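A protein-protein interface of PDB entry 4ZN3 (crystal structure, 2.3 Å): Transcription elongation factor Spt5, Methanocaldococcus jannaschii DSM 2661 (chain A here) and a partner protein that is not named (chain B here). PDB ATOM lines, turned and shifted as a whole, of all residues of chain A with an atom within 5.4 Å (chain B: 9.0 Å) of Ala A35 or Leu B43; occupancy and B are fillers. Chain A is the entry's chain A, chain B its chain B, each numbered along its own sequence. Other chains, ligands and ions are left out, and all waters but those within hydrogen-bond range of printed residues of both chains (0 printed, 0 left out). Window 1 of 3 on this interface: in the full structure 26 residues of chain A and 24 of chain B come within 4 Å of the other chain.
Among the printed residues, merely in contact across the chains: Glu A37 with Ile B41 (3.2 Å), Ala A16 with Ile B45 (3.4 Å), Leu A34 with Leu B43 (3.4 Å), Ile A33 with Leu B44 (3.5 Å), Ala A35 with Gly B42 (3.7 Å), Lys A13 with Leu B43 (3.7 Å), Gly A17 with Ile B45 (3.8 Å), Ile A33 with Leu B43 (3.8 Å), Ala A16 with Leu B43 (3.9 Å) and Leu A34 with Ile B54 (3.999 Å).
The side-chain amino group (NZ) of Lys A13 is in salt-bridge range of the side-chain carboxylate (OE1) of Glu A37 (3.4 Å). The backbone carbonyl oxygen of Ser B69 lies within hydrogen-bond range of the backbone NH of Ile B41, at 3.1 Å. The backbone carbonyl oxygen of Leu A44 is in hydrogen-bond range of the backbone NH of Leu A34, at 2.7 Å. O of Gly B42 is in hydrogen-bond range of N of Leu B68, 3.3 Å away. The backbone NH of Tyr B66 lies within hydrogen-bond range of the backbone carbonyl oxygen of Leu B44 (2.8 Å). The backbone NH (N) of Leu B68 is in hydrogen-bond range of the backbone carbonyl oxygen (O) of Ile B41, at 3.0 Å.
Printed residues of chain B that touch a printed residue of chain A: Ile B41, Gly B42, Leu B43, Leu B44, Ile B45 and Ile B54. Hydrophobic or aromatic side chains of chain B that line the printed part of chain A: Ile B41, Leu B43, Leu B44, Ile B45 and Ile B54. Among the printed residues, 13 pairs touch across the chains. Among the printed residues, no Asp or Glu carboxylate lies within 4 Å of a Lys or Arg side-chain nitrogen of the other chain.
Of the printed residues of chain B, Ala A16 touches Leu B43 (3.9 Å) and Ile B45 (3.4 Å). Of chain B, only Gly B42 (3.7 Å) and Leu B43 (2.8 Å) come within 4 Å of Ala A35. No residue of chain B comes within 4 Å of Ser A36. Leu B43 touches just these residues of chain A: Lys A13, Ala A16, Ile A33, Leu A34 and Ala A35. Of the printed residues of chain A, Ile B54 touches Leu A34.
N of Gly B42 lies within hydrogen-bond range of OE1 of Glu A37 (2.9 Å). The backbone NH (N) of Ile B45 is in hydrogen-bond range of the backbone carbonyl oxygen (O) of Ile A33 (2.8 Å). The backbone NH of Ala A35 sits at hydrogen-bond distance from the backbone carbonyl oxygen of Leu B43.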
ATOM      1  N   GLU A  12     -22.955 -33.344  23.933  1.00  0.00           N
ATOM      2  CA  GLU A  12     -22.234 -32.217  24.533  1.00  0.00           C
ATOM      3  C   GLU A  12     -23.214 -31.184  25.077  1.00  0.00           C
ATOM      4  O   GLU A  12     -23.088 -30.740  26.216  1.00  0.00           O
ATOM      5  CB  GLU A  12     -21.278 -31.564  23.525  1.00  0.00           C
ATOM      6  CG  GLU A  12     -20.210 -32.506  22.966  1.00  0.00           C
ATOM      7  CD  GLU A  12     -20.642 -33.279  21.724  1.00  0.00           C
ATOM      8  OE1 GLU A  12     -21.837 -33.266  21.362  1.00  0.00           O
ATOM      9  OE2 GLU A  12     -19.774 -33.926  21.104  1.00  0.00           O
ATOM     10  N   LYS A  13     -24.195 -30.828  24.257  1.00  0.00           N
ATOM     11  CA  LYS A  13     -25.229 -29.870  24.649  1.00  0.00           C
ATOM     12  C   LYS A  13     -26.080 -30.364  25.826  1.00  0.00           C
ATOM     13  O   LYS A  13     -26.406 -29.581  26.724  1.00  0.00           O
ATOM     14  CB  LYS A  13     -26.123 -29.521  23.455  1.00  0.00           C
ATOM     15  CG  LYS A  13     -25.418 -28.731  22.362  1.00  0.00           C
ATOM     16  CD  LYS A  13     -26.378 -28.365  21.239  1.00  0.00           C
ATOM     17  CE  LYS A  13     -25.652 -28.092  19.929  1.00  0.00           C
ATOM     18  NZ  LYS A  13     -25.299 -29.350  19.210  1.00  0.00           N
ATOM     19  N   ALA A  16     -23.903 -30.269  28.983  1.00  0.00           N
ATOM     20  CA  ALA A  16     -23.775 -28.855  29.344  1.00  0.00           C
ATOM     21  C   ALA A  16     -25.006 -28.375  30.104  1.00  0.00           C
ATOM     22  O   ALA A  16     -24.886 -27.673  31.112  1.00  0.00           O
ATOM     23  CB  ALA A  16     -23.545 -27.996  28.109  1.00  0.00           C
ATOM     24  N   GLY A  17     -26.185 -28.762  29.623  1.00  0.00           N
ATOM     25  CA  GLY A  17     -27.438 -28.473  30.319  1.00  0.00           C
ATOM     26  C   GLY A  17     -27.477 -29.064  31.718  1.00  0.00           C
ATOM     27  O   GLY A  17     -27.821 -28.375  32.674  1.00  0.00           O
ATOM     28  N   ILE A  33     -20.435 -22.538  30.585  1.00  0.00           N
ATOM     29  CA  ILE A  33     -20.192 -23.829  29.956  1.00  0.00           C
ATOM     30  C   ILE A  33     -20.310 -23.641  28.446  1.00  0.00           C
ATOM     31  O   ILE A  33     -21.323 -23.130  27.968  1.00  0.00           O
ATOM     32  CB  ILE A  33     -21.202 -24.895  30.424  1.00  0.00           C
ATOM     33  CG1 ILE A  33     -21.128 -25.098  31.944  1.00  0.00           C
ATOM     34  CG2 ILE A  33     -20.936 -26.220  29.723  1.00  0.00           C
ATOM     35  CD1 ILE A  33     -22.358 -25.761  32.521  1.00  0.00           C
ATOM     36  N   LEU A  34     -19.286 -24.064  27.707  1.00  0.00           N
ATOM     37  CA  LEU A  34     -19.240 -23.913  26.253  1.00  0.00           C
ATOM     38  C   LEU A  34     -19.165 -25.281  25.585  1.00  0.00           C
ATOM     39  O   LEU A  34     -18.287 -26.083  25.903  1.00  0.00           O
ATOM     40  CB  LEU A  34     -18.035 -23.062  25.852  1.00  0.00           C
ATOM     41  CG  LEU A  34     -18.105 -22.324  24.506  1.00  0.00           C
ATOM     42  CD1 LEU A  34     -17.057 -21.219  24.454  1.00  0.00           C
ATOM     43  CD2 LEU A  34     -17.922 -23.267  23.332  1.00  0.00           C
ATOM     44  N   ALA A  35     -20.100 -25.543  24.675  1.00  0.00           N
ATOM     45  CA  ALA A  35     -20.069 -26.730  23.826  1.00  0.00           C
ATOM     46  C   ALA A  35     -20.005 -26.250  22.389  1.00  0.00           C
ATOM     47  O   ALA A  35     -20.995 -25.754  21.852  1.00  0.00           O
ATOM     48  CB  ALA A  35     -21.299 -27.597  24.051  1.00  0.00           C
ATOM     49  N   SER A  36     -18.822 -26.370  21.790  1.00  0.00           N
ATOM     50  CA  SER A  36     -18.588 -25.994  20.396  1.00  0.00           C
ATOM     51  C   SER A  36     -18.679 -27.233  19.516  1.00  0.00           C
ATOM     52  O   SER A  36     -18.176 -28.292  19.883  1.00  0.00           O
ATOM     53  CB  SER A  36     -17.200 -25.360  20.245  1.00  0.00           C
ATOM     54  OG  SER A  36     -16.923 -25.029  18.889  1.00  0.00           O
ATOM     55  N   GLU A  37     -19.290 -27.101  18.342  1.00  0.00           N
ATOM     56  CA  GLU A  37     -19.320 -28.212  17.375  1.00  0.00           C
ATOM     57  C   GLU A  37     -17.956 -28.448  16.697  1.00  0.00           C
ATOM     58  O   GLU A  37     -17.743 -29.499  16.099  1.00  0.00           O
ATOM     59  CB  GLU A  37     -20.468 -28.037  16.369  1.00  0.00           C
ATOM     60  CG  GLU A  37     -21.812 -28.476  16.959  1.00  0.00           C
ATOM     61  CD  GLU A  37     -23.014 -27.770  16.358  1.00  0.00           C
ATOM     62  OE1 GLU A  37     -23.758 -27.101  17.114  1.00  0.00           O
ATOM     63  OE2 GLU A  37     -23.221 -27.886  15.134  1.00  0.00           O
ATOM     64  N   TYR A  42     -16.183 -32.838  23.679  1.00  0.00           N
ATOM     65  CA  TYR A  42     -15.625 -31.948  24.703  1.00  0.00           C
ATOM     66  C   TYR A  42     -16.580 -30.818  25.072  1.00  0.00           C
ATOM     67  O   TYR A  42     -17.221 -30.222  24.212  1.00  0.00           O
ATOM     68  CB  TYR A  42     -14.299 -31.347  24.239  1.00  0.00           C
ATOM     69  CG  TYR A  42     -13.176 -32.345  24.160  1.00  0.00           C
ATOM     70  CD1 TYR A  42     -12.413 -32.654  25.281  1.00  0.00           C
ATOM     71  CD2 TYR A  42     -12.877 -32.988  22.963  1.00  0.00           C
ATOM     72  CE1 TYR A  42     -11.373 -33.568  25.209  1.00  0.00           C
ATOM     73  CE2 TYR A  42     -11.845 -33.911  22.880  1.00  0.00           C
ATOM     74  CZ  TYR A  42     -11.095 -34.195  24.006  1.00  0.00           C
ATOM     75  OH  TYR A  42     -10.067 -35.103  23.934  1.00  0.00           O
ATOM     76  N   VAL A  43     -16.654 -30.537  26.367  1.00  0.00           N
ATOM     77  CA  VAL A  43     -17.405 -29.413  26.892  1.00  0.00           C
ATOM     78  C   VAL A  43     -16.432 -28.610  27.740  1.00  0.00           C
ATOM     79  O   VAL A  43     -15.714 -29.183  28.564  1.00  0.00           O
ATOM     80  CB  VAL A  43     -18.612 -29.908  27.723  1.00  0.00           C
ATOM     81  CG1 VAL A  43     -19.164 -28.819  28.626  1.00  0.00           C
ATOM     82  CG2 VAL A  43     -19.699 -30.421  26.795  1.00  0.00           C
ATOM     83  N   LEU A  44     -16.405 -27.296  27.531  1.00  0.00           N
ATOM     84  CA  LEU A  44     -15.539 -26.401  28.292  1.00  0.00           C
ATOM     85  C   LEU A  44     -16.322 -25.817  29.453  1.00  0.00           C
ATOM     86  O   LEU A  44     -17.398 -25.252  29.248  1.00  0.00           O
ATOM     87  CB  LEU A  44     -15.003 -25.270  27.409  1.00  0.00           C
ATOM     88  CG  LEU A  44     -14.207 -25.688  26.165  1.00  0.00           C
ATOM     89  CD1 LEU A  44     -13.717 -24.460  25.415  1.00  0.00           C
ATOM     90  CD2 LEU A  44     -13.035 -26.586  26.528  1.00  0.00           C
ATOM     91  N   PRO B  14     -34.917 -25.939  20.884  1.00  0.00           N
ATOM     92  CA  PRO B  14     -35.098 -24.495  20.999  1.00  0.00           C
ATOM     93  C   PRO B  14     -34.646 -23.729  19.752  1.00  0.00           C
ATOM     94  O   PRO B  14     -33.803 -24.202  18.988  1.00  0.00           O
ATOM     95  CB  PRO B  14     -34.242 -24.125  22.213  1.00  0.00           C
ATOM     96  CG  PRO B  14     -33.188 -25.167  22.271  1.00  0.00           C
ATOM     97  CD  PRO B  14     -33.763 -26.419  21.669  1.00  0.00           C
ATOM     98  N   LYS B  21     -28.977 -14.030  20.298  1.00  0.00           N
ATOM     99  CA  LYS B  21     -28.662 -15.483  20.317  1.00  0.00           C
ATOM    100  C   LYS B  21     -29.238 -16.318  21.483  1.00  0.00           C
ATOM    101  O   LYS B  21     -29.008 -17.527  21.547  1.00  0.00           O
ATOM    102  CB  LYS B  21     -27.153 -15.726  20.142  1.00  0.00           C
ATOM    103  CG  LYS B  21     -26.631 -15.240  18.797  1.00  0.00           C
ATOM    104  CD  LYS B  21     -25.115 -15.312  18.693  1.00  0.00           C
ATOM    105  CE  LYS B  21     -24.440 -14.140  19.386  1.00  0.00           C
ATOM    106  NZ  LYS B  21     -22.997 -14.064  19.030  1.00  0.00           N
ATOM    107  N   TYR B  22     -30.025 -15.684  22.351  1.00  0.00           N
ATOM    108  CA  TYR B  22     -30.670 -16.339  23.489  1.00  0.00           C
ATOM    109  C   TYR B  22     -31.578 -17.479  23.020  1.00  0.00           C
ATOM    110  O   TYR B  22     -32.356 -17.305  22.078  1.00  0.00           O
ATOM    111  CB  TYR B  22     -31.480 -15.292  24.263  1.00  0.00           C
ATOM    112  CG  TYR B  22     -32.138 -15.774  25.535  1.00  0.00           C
ATOM    113  CD1 TYR B  22     -31.444 -15.772  26.740  1.00  0.00           C
ATOM    114  CD2 TYR B  22     -33.468 -16.194  25.542  1.00  0.00           C
ATOM    115  CE1 TYR B  22     -32.045 -16.192  27.914  1.00  0.00           C
ATOM    116  CE2 TYR B  22     -34.078 -16.621  26.713  1.00  0.00           C
ATOM    117  CZ  TYR B  22     -33.361 -16.618  27.894  1.00  0.00           C
ATOM    118  OH  TYR B  22     -33.951 -17.036  29.060  1.00  0.00           O
ATOM    119  N   LEU B  23     -31.466 -18.639  23.668  1.00  0.00           N
ATOM    120  CA  LEU B  23     -32.260 -19.813  23.297  1.00  0.00           C
ATOM    121  C   LEU B  23     -33.654 -19.778  23.924  1.00  0.00           C
ATOM    122  O   LEU B  23     -33.814 -19.407  25.086  1.00  0.00           O
ATOM    123  CB  LEU B  23     -31.538 -21.116  23.676  1.00  0.00           C
ATOM    124  CG  LEU B  23     -30.166 -21.374  23.029  1.00  0.00           C
ATOM    125  CD1 LEU B  23     -29.664 -22.761  23.403  1.00  0.00           C
ATOM    126  CD2 LEU B  23     -30.191 -21.226  21.510  1.00  0.00           C
ATOM    127  N   TRP B  40     -29.360 -22.460  14.001  1.00  0.00           N
ATOM    128  CA  TRP B  40     -28.267 -22.052  14.896  1.00  0.00           C
ATOM    129  C   TRP B  40     -27.360 -23.219  15.266  1.00  0.00           C
ATOM    130  O   TRP B  40     -27.760 -24.382  15.169  1.00  0.00           O
ATOM    131  CB  TRP B  40     -28.830 -21.405  16.174  1.00  0.00           C
ATOM    132  CG  TRP B  40     -29.662 -22.328  17.047  1.00  0.00           C
ATOM    133  CD1 TRP B  40     -31.013 -22.509  16.987  1.00  0.00           C
ATOM    134  CD2 TRP B  40     -29.192 -23.178  18.108  1.00  0.00           C
ATOM    135  NE1 TRP B  40     -31.416 -23.420  17.937  1.00  0.00           N
ATOM    136  CE2 TRP B  40     -30.319 -23.848  18.638  1.00  0.00           C
ATOM    137  CE3 TRP B  40     -27.928 -23.443  18.659  1.00  0.00           C
ATOM    138  CZ2 TRP B  40     -30.223 -24.767  19.695  1.00  0.00           C
ATOM    139  CZ3 TRP B  40     -27.835 -24.360  19.717  1.00  0.00           C
ATOM    140  CH2 TRP B  40     -28.980 -25.008  20.220  1.00  0.00           C
ATOM    141  N   ILE B  41     -26.143 -22.892  15.703  1.00  0.00           N
ATOM    142  CA  ILE B  41     -25.173 -23.896  16.168  1.00  0.00           C
ATOM    143  C   ILE B  41     -24.360 -23.407  17.368  1.00  0.00           C
ATOM    144  O   ILE B  41     -24.215 -22.199  17.602  1.00  0.00           O
ATOM    145  CB  ILE B  41     -24.209 -24.383  15.044  1.00  0.00           C
ATOM    146  CG1 ILE B  41     -23.616 -23.216  14.237  1.00  0.00           C
ATOM    147  CG2 ILE B  41     -24.915 -25.356  14.107  1.00  0.00           C
ATOM    148  CD1 ILE B  41     -22.386 -22.584  14.846  1.00  0.00           C
ATOM    149  N   GLY B  42     -23.840 -24.370  18.125  1.00  0.00           N
ATOM    150  CA  GLY B  42     -23.011 -24.095  19.286  1.00  0.00           C
ATOM    151  C   GLY B  42     -23.828 -23.670  20.487  1.00  0.00           C
ATOM    152  O   GLY B  42     -24.900 -23.096  20.348  1.00  0.00           O
ATOM    153  N   LEU B  43     -23.299 -23.942  21.674  1.00  0.00           N
ATOM    154  CA  LEU B  43     -23.983 -23.644  22.925  1.00  0.00           C
ATOM    155  C   LEU B  43     -23.025 -22.977  23.899  1.00  0.00           C
ATOM    156  O   LEU B  43     -21.962 -23.518  24.200  1.00  0.00           O
ATOM    157  CB  LEU B  43     -24.538 -24.928  23.534  1.00  0.00           C
ATOM    158  CG  LEU B  43     -25.237 -24.836  24.893  1.00  0.00           C
ATOM    159  CD1 LEU B  43     -26.469 -23.942  24.827  1.00  0.00           C
ATOM    160  CD2 LEU B  43     -25.602 -26.235  25.364  1.00  0.00           C
ATOM    161  N   LEU B  44     -23.408 -21.799  24.376  1.00  0.00           N
ATOM    162  CA  LEU B  44     -22.734 -21.142  25.487  1.00  0.00           C
ATOM    163  C   LEU B  44     -23.776 -20.918  26.571  1.00  0.00           C
ATOM    164  O   LEU B  44     -24.745 -20.189  26.359  1.00  0.00           O
ATOM    165  CB  LEU B  44     -22.124 -19.812  25.044  1.00  0.00           C
ATOM    166  CG  LEU B  44     -21.460 -18.929  26.109  1.00  0.00           C
ATOM    167  CD1 LEU B  44     -20.418 -19.680  26.928  1.00  0.00           C
ATOM    168  CD2 LEU B  44     -20.830 -17.712  25.450  1.00  0.00           C
ATOM    169  N   ILE B  45     -23.586 -21.572  27.716  1.00  0.00           N
ATOM    170  CA  ILE B  45     -24.443 -21.366  28.880  1.00  0.00           C
ATOM    171  C   ILE B  45     -23.723 -20.419  29.821  1.00  0.00           C
ATOM    172  O   ILE B  45     -22.695 -20.774  30.389  1.00  0.00           O
ATOM    173  CB  ILE B  45     -24.771 -22.690  29.602  1.00  0.00           C
ATOM    174  CG1 ILE B  45     -25.445 -23.668  28.625  1.00  0.00           C
ATOM    175  CG2 ILE B  45     -25.667 -22.428  30.809  1.00  0.00           C
ATOM    176  CD1 ILE B  45     -25.805 -25.012  29.221  1.00  0.00           C
ATOM    177  N   VAL B  46     -24.269 -19.216  29.976  1.00  0.00           N
ATOM    178  CA  VAL B  46     -23.739 -18.231  30.910  1.00  0.00           C
ATOM    179  C   VAL B  46     -24.506 -18.380  32.215  1.00  0.00           C
ATOM    180  O   VAL B  46     -25.704 -18.095  32.266  1.00  0.00           O
ATOM    181  CB  VAL B  46     -23.882 -16.793  30.363  1.00  0.00           C
ATOM    182  CG1 VAL B  46     -23.336 -15.778  31.361  1.00  0.00           C
ATOM    183  CG2 VAL B  46     -23.154 -16.671  29.035  1.00  0.00           C
ATOM    184  N   ILE B  54     -15.566 -15.798  29.582  1.00  0.00           N
ATOM    185  CA  ILE B  54     -16.139 -16.279  28.318  1.00  0.00           C
ATOM    186  C   ILE B  54     -17.331 -15.402  27.922  1.00  0.00           C
ATOM    187  O   ILE B  54     -17.431 -14.974  26.776  1.00  0.00           O
ATOM    188  CB  ILE B  54     -16.554 -17.772  28.356  1.00  0.00           C
ATOM    189  CG1 ILE B  54     -15.317 -18.652  28.605  1.00  0.00           C
ATOM    190  CG2 ILE B  54     -17.225 -18.173  27.040  1.00  0.00           C
ATOM    191  CD1 ILE B  54     -15.551 -20.152  28.580  1.00  0.00           C
ATOM    192  N   ILE B  60     -21.896 -11.019  26.422  1.00  0.00           N
ATOM    193  CA  ILE B  60     -23.126 -11.455  27.078  1.00  0.00           C
ATOM    194  C   ILE B  60     -23.102 -11.005  28.538  1.00  0.00           C
ATOM    195  O   ILE B  60     -22.208 -11.393  29.291  1.00  0.00           O
ATOM    196  CB  ILE B  60     -23.291 -12.989  26.998  1.00  0.00           C
ATOM    197  CG1 ILE B  60     -23.467 -13.419  25.531  1.00  0.00           C
ATOM    198  CG2 ILE B  60     -24.482 -13.447  27.842  1.00  0.00           C
ATOM    199  CD1 ILE B  60     -23.352 -14.911  25.286  1.00  0.00           C
ATOM    200  N   GLY B  64     -28.141 -17.125  30.885  1.00  0.00           N
ATOM    201  CA  GLY B  64     -28.995 -17.920  30.010  1.00  0.00           C
ATOM    202  C   GLY B  64     -28.188 -18.774  29.058  1.00  0.00           C
ATOM    203  O   GLY B  64     -26.956 -18.753  29.084  1.00  0.00           O
ATOM    204  N   LYS B  65     -28.901 -19.536  28.232  1.00  0.00           N
ATOM    205  CA  LYS B  65     -28.296 -20.374  27.207  1.00  0.00           C
ATOM    206  C   LYS B  65     -28.329 -19.635  25.892  1.00  0.00           C
ATOM    207  O   LYS B  65     -29.347 -19.044  25.533  1.00  0.00           O
ATOM    208  CB  LYS B  65     -29.064 -21.675  27.045  1.00  0.00           C
ATOM    209  CG  LYS B  65     -29.290 -22.443  28.328  1.00  0.00           C
ATOM    210  CD  LYS B  65     -29.754 -23.851  27.989  1.00  0.00           C
ATOM    211  CE  LYS B  65     -30.727 -24.423  29.004  1.00  0.00           C
ATOM    212  NZ  LYS B  65     -29.999 -24.973  30.172  1.00  0.00           N
ATOM    213  N   TYR B  66     -27.224 -19.699  25.161  1.00  0.00           N
ATOM    214  CA  TYR B  66     -27.066 -18.958  23.918  1.00  0.00           C
ATOM    215  C   TYR B  66     -26.488 -19.834  22.831  1.00  0.00           C
ATOM    216  O   TYR B  66     -25.659 -20.702  23.106  1.00  0.00           O
ATOM    217  CB  TYR B  66     -26.108 -17.791  24.132  1.00  0.00           C
ATOM    218  CG  TYR B  66     -26.627 -16.727  25.053  1.00  0.00           C
ATOM    219  CD1 TYR B  66     -26.539 -16.871  26.437  1.00  0.00           C
ATOM    220  CD2 TYR B  66     -27.186 -15.560  24.545  1.00  0.00           C
ATOM    221  CE1 TYR B  66     -27.009 -15.888  27.288  1.00  0.00           C
ATOM    222  CE2 TYR B  66     -27.659 -14.568  25.387  1.00  0.00           C
ATOM    223  CZ  TYR B  66     -27.570 -14.737  26.754  1.00  0.00           C
ATOM    224  OH  TYR B  66     -28.039 -13.752  27.584  1.00  0.00           O
ATOM    225  N   ALA B  67     -26.912 -19.580  21.597  1.00  0.00           N
ATOM    226  CA  ALA B  67     -26.227 -20.103  20.419  1.00  0.00           C
ATOM    227  C   ALA B  67     -24.897 -19.369  20.241  1.00  0.00           C
ATOM    228  O   ALA B  67     -24.756 -18.223  20.674  1.00  0.00           O
ATOM    229  CB  ALA B  67     -27.091 -19.929  19.178  1.00  0.00           C
ATOM    230  N   LEU B  68     -23.926 -20.024  19.616  1.00  0.00           N
ATOM    231  CA  LEU B  68     -22.681 -19.348  19.229  1.00  0.00           C
ATOM    232  C   LEU B  68     -22.880 -18.539  17.954  1.00  0.00           C
ATOM    233  O   LEU B  68     -22.331 -17.447  17.835  1.00  0.00           O
ATOM    234  CB  LEU B  68     -21.541 -20.345  19.055  1.00  0.00           C
ATOM    235  CG  LEU B  68     -21.147 -21.104  20.319  1.00  0.00           C
ATOM    236  CD1 LEU B  68     -19.976 -22.018  20.004  1.00  0.00           C
ATOM    237  CD2 LEU B  68     -20.806 -20.172  21.474  1.00  0.00           C
ATOM    238  N   SER B  69     -23.651 -19.076  17.007  1.00  0.00           N
ATOM    239  CA  SER B  69     -24.115 -18.297  15.852  1.00  0.00           C
ATOM    240  C   SER B  69     -25.524 -18.684  15.399  1.00  0.00           C
ATOM    241  O   SER B  69     -25.977 -19.812  15.610  1.00  0.00           O
ATOM    242  CB  SER B  69     -23.152 -18.438  14.676  1.00  0.00           C
ATOM    243  OG  SER B  69     -23.263 -19.717  14.083  1.00  0.00           O
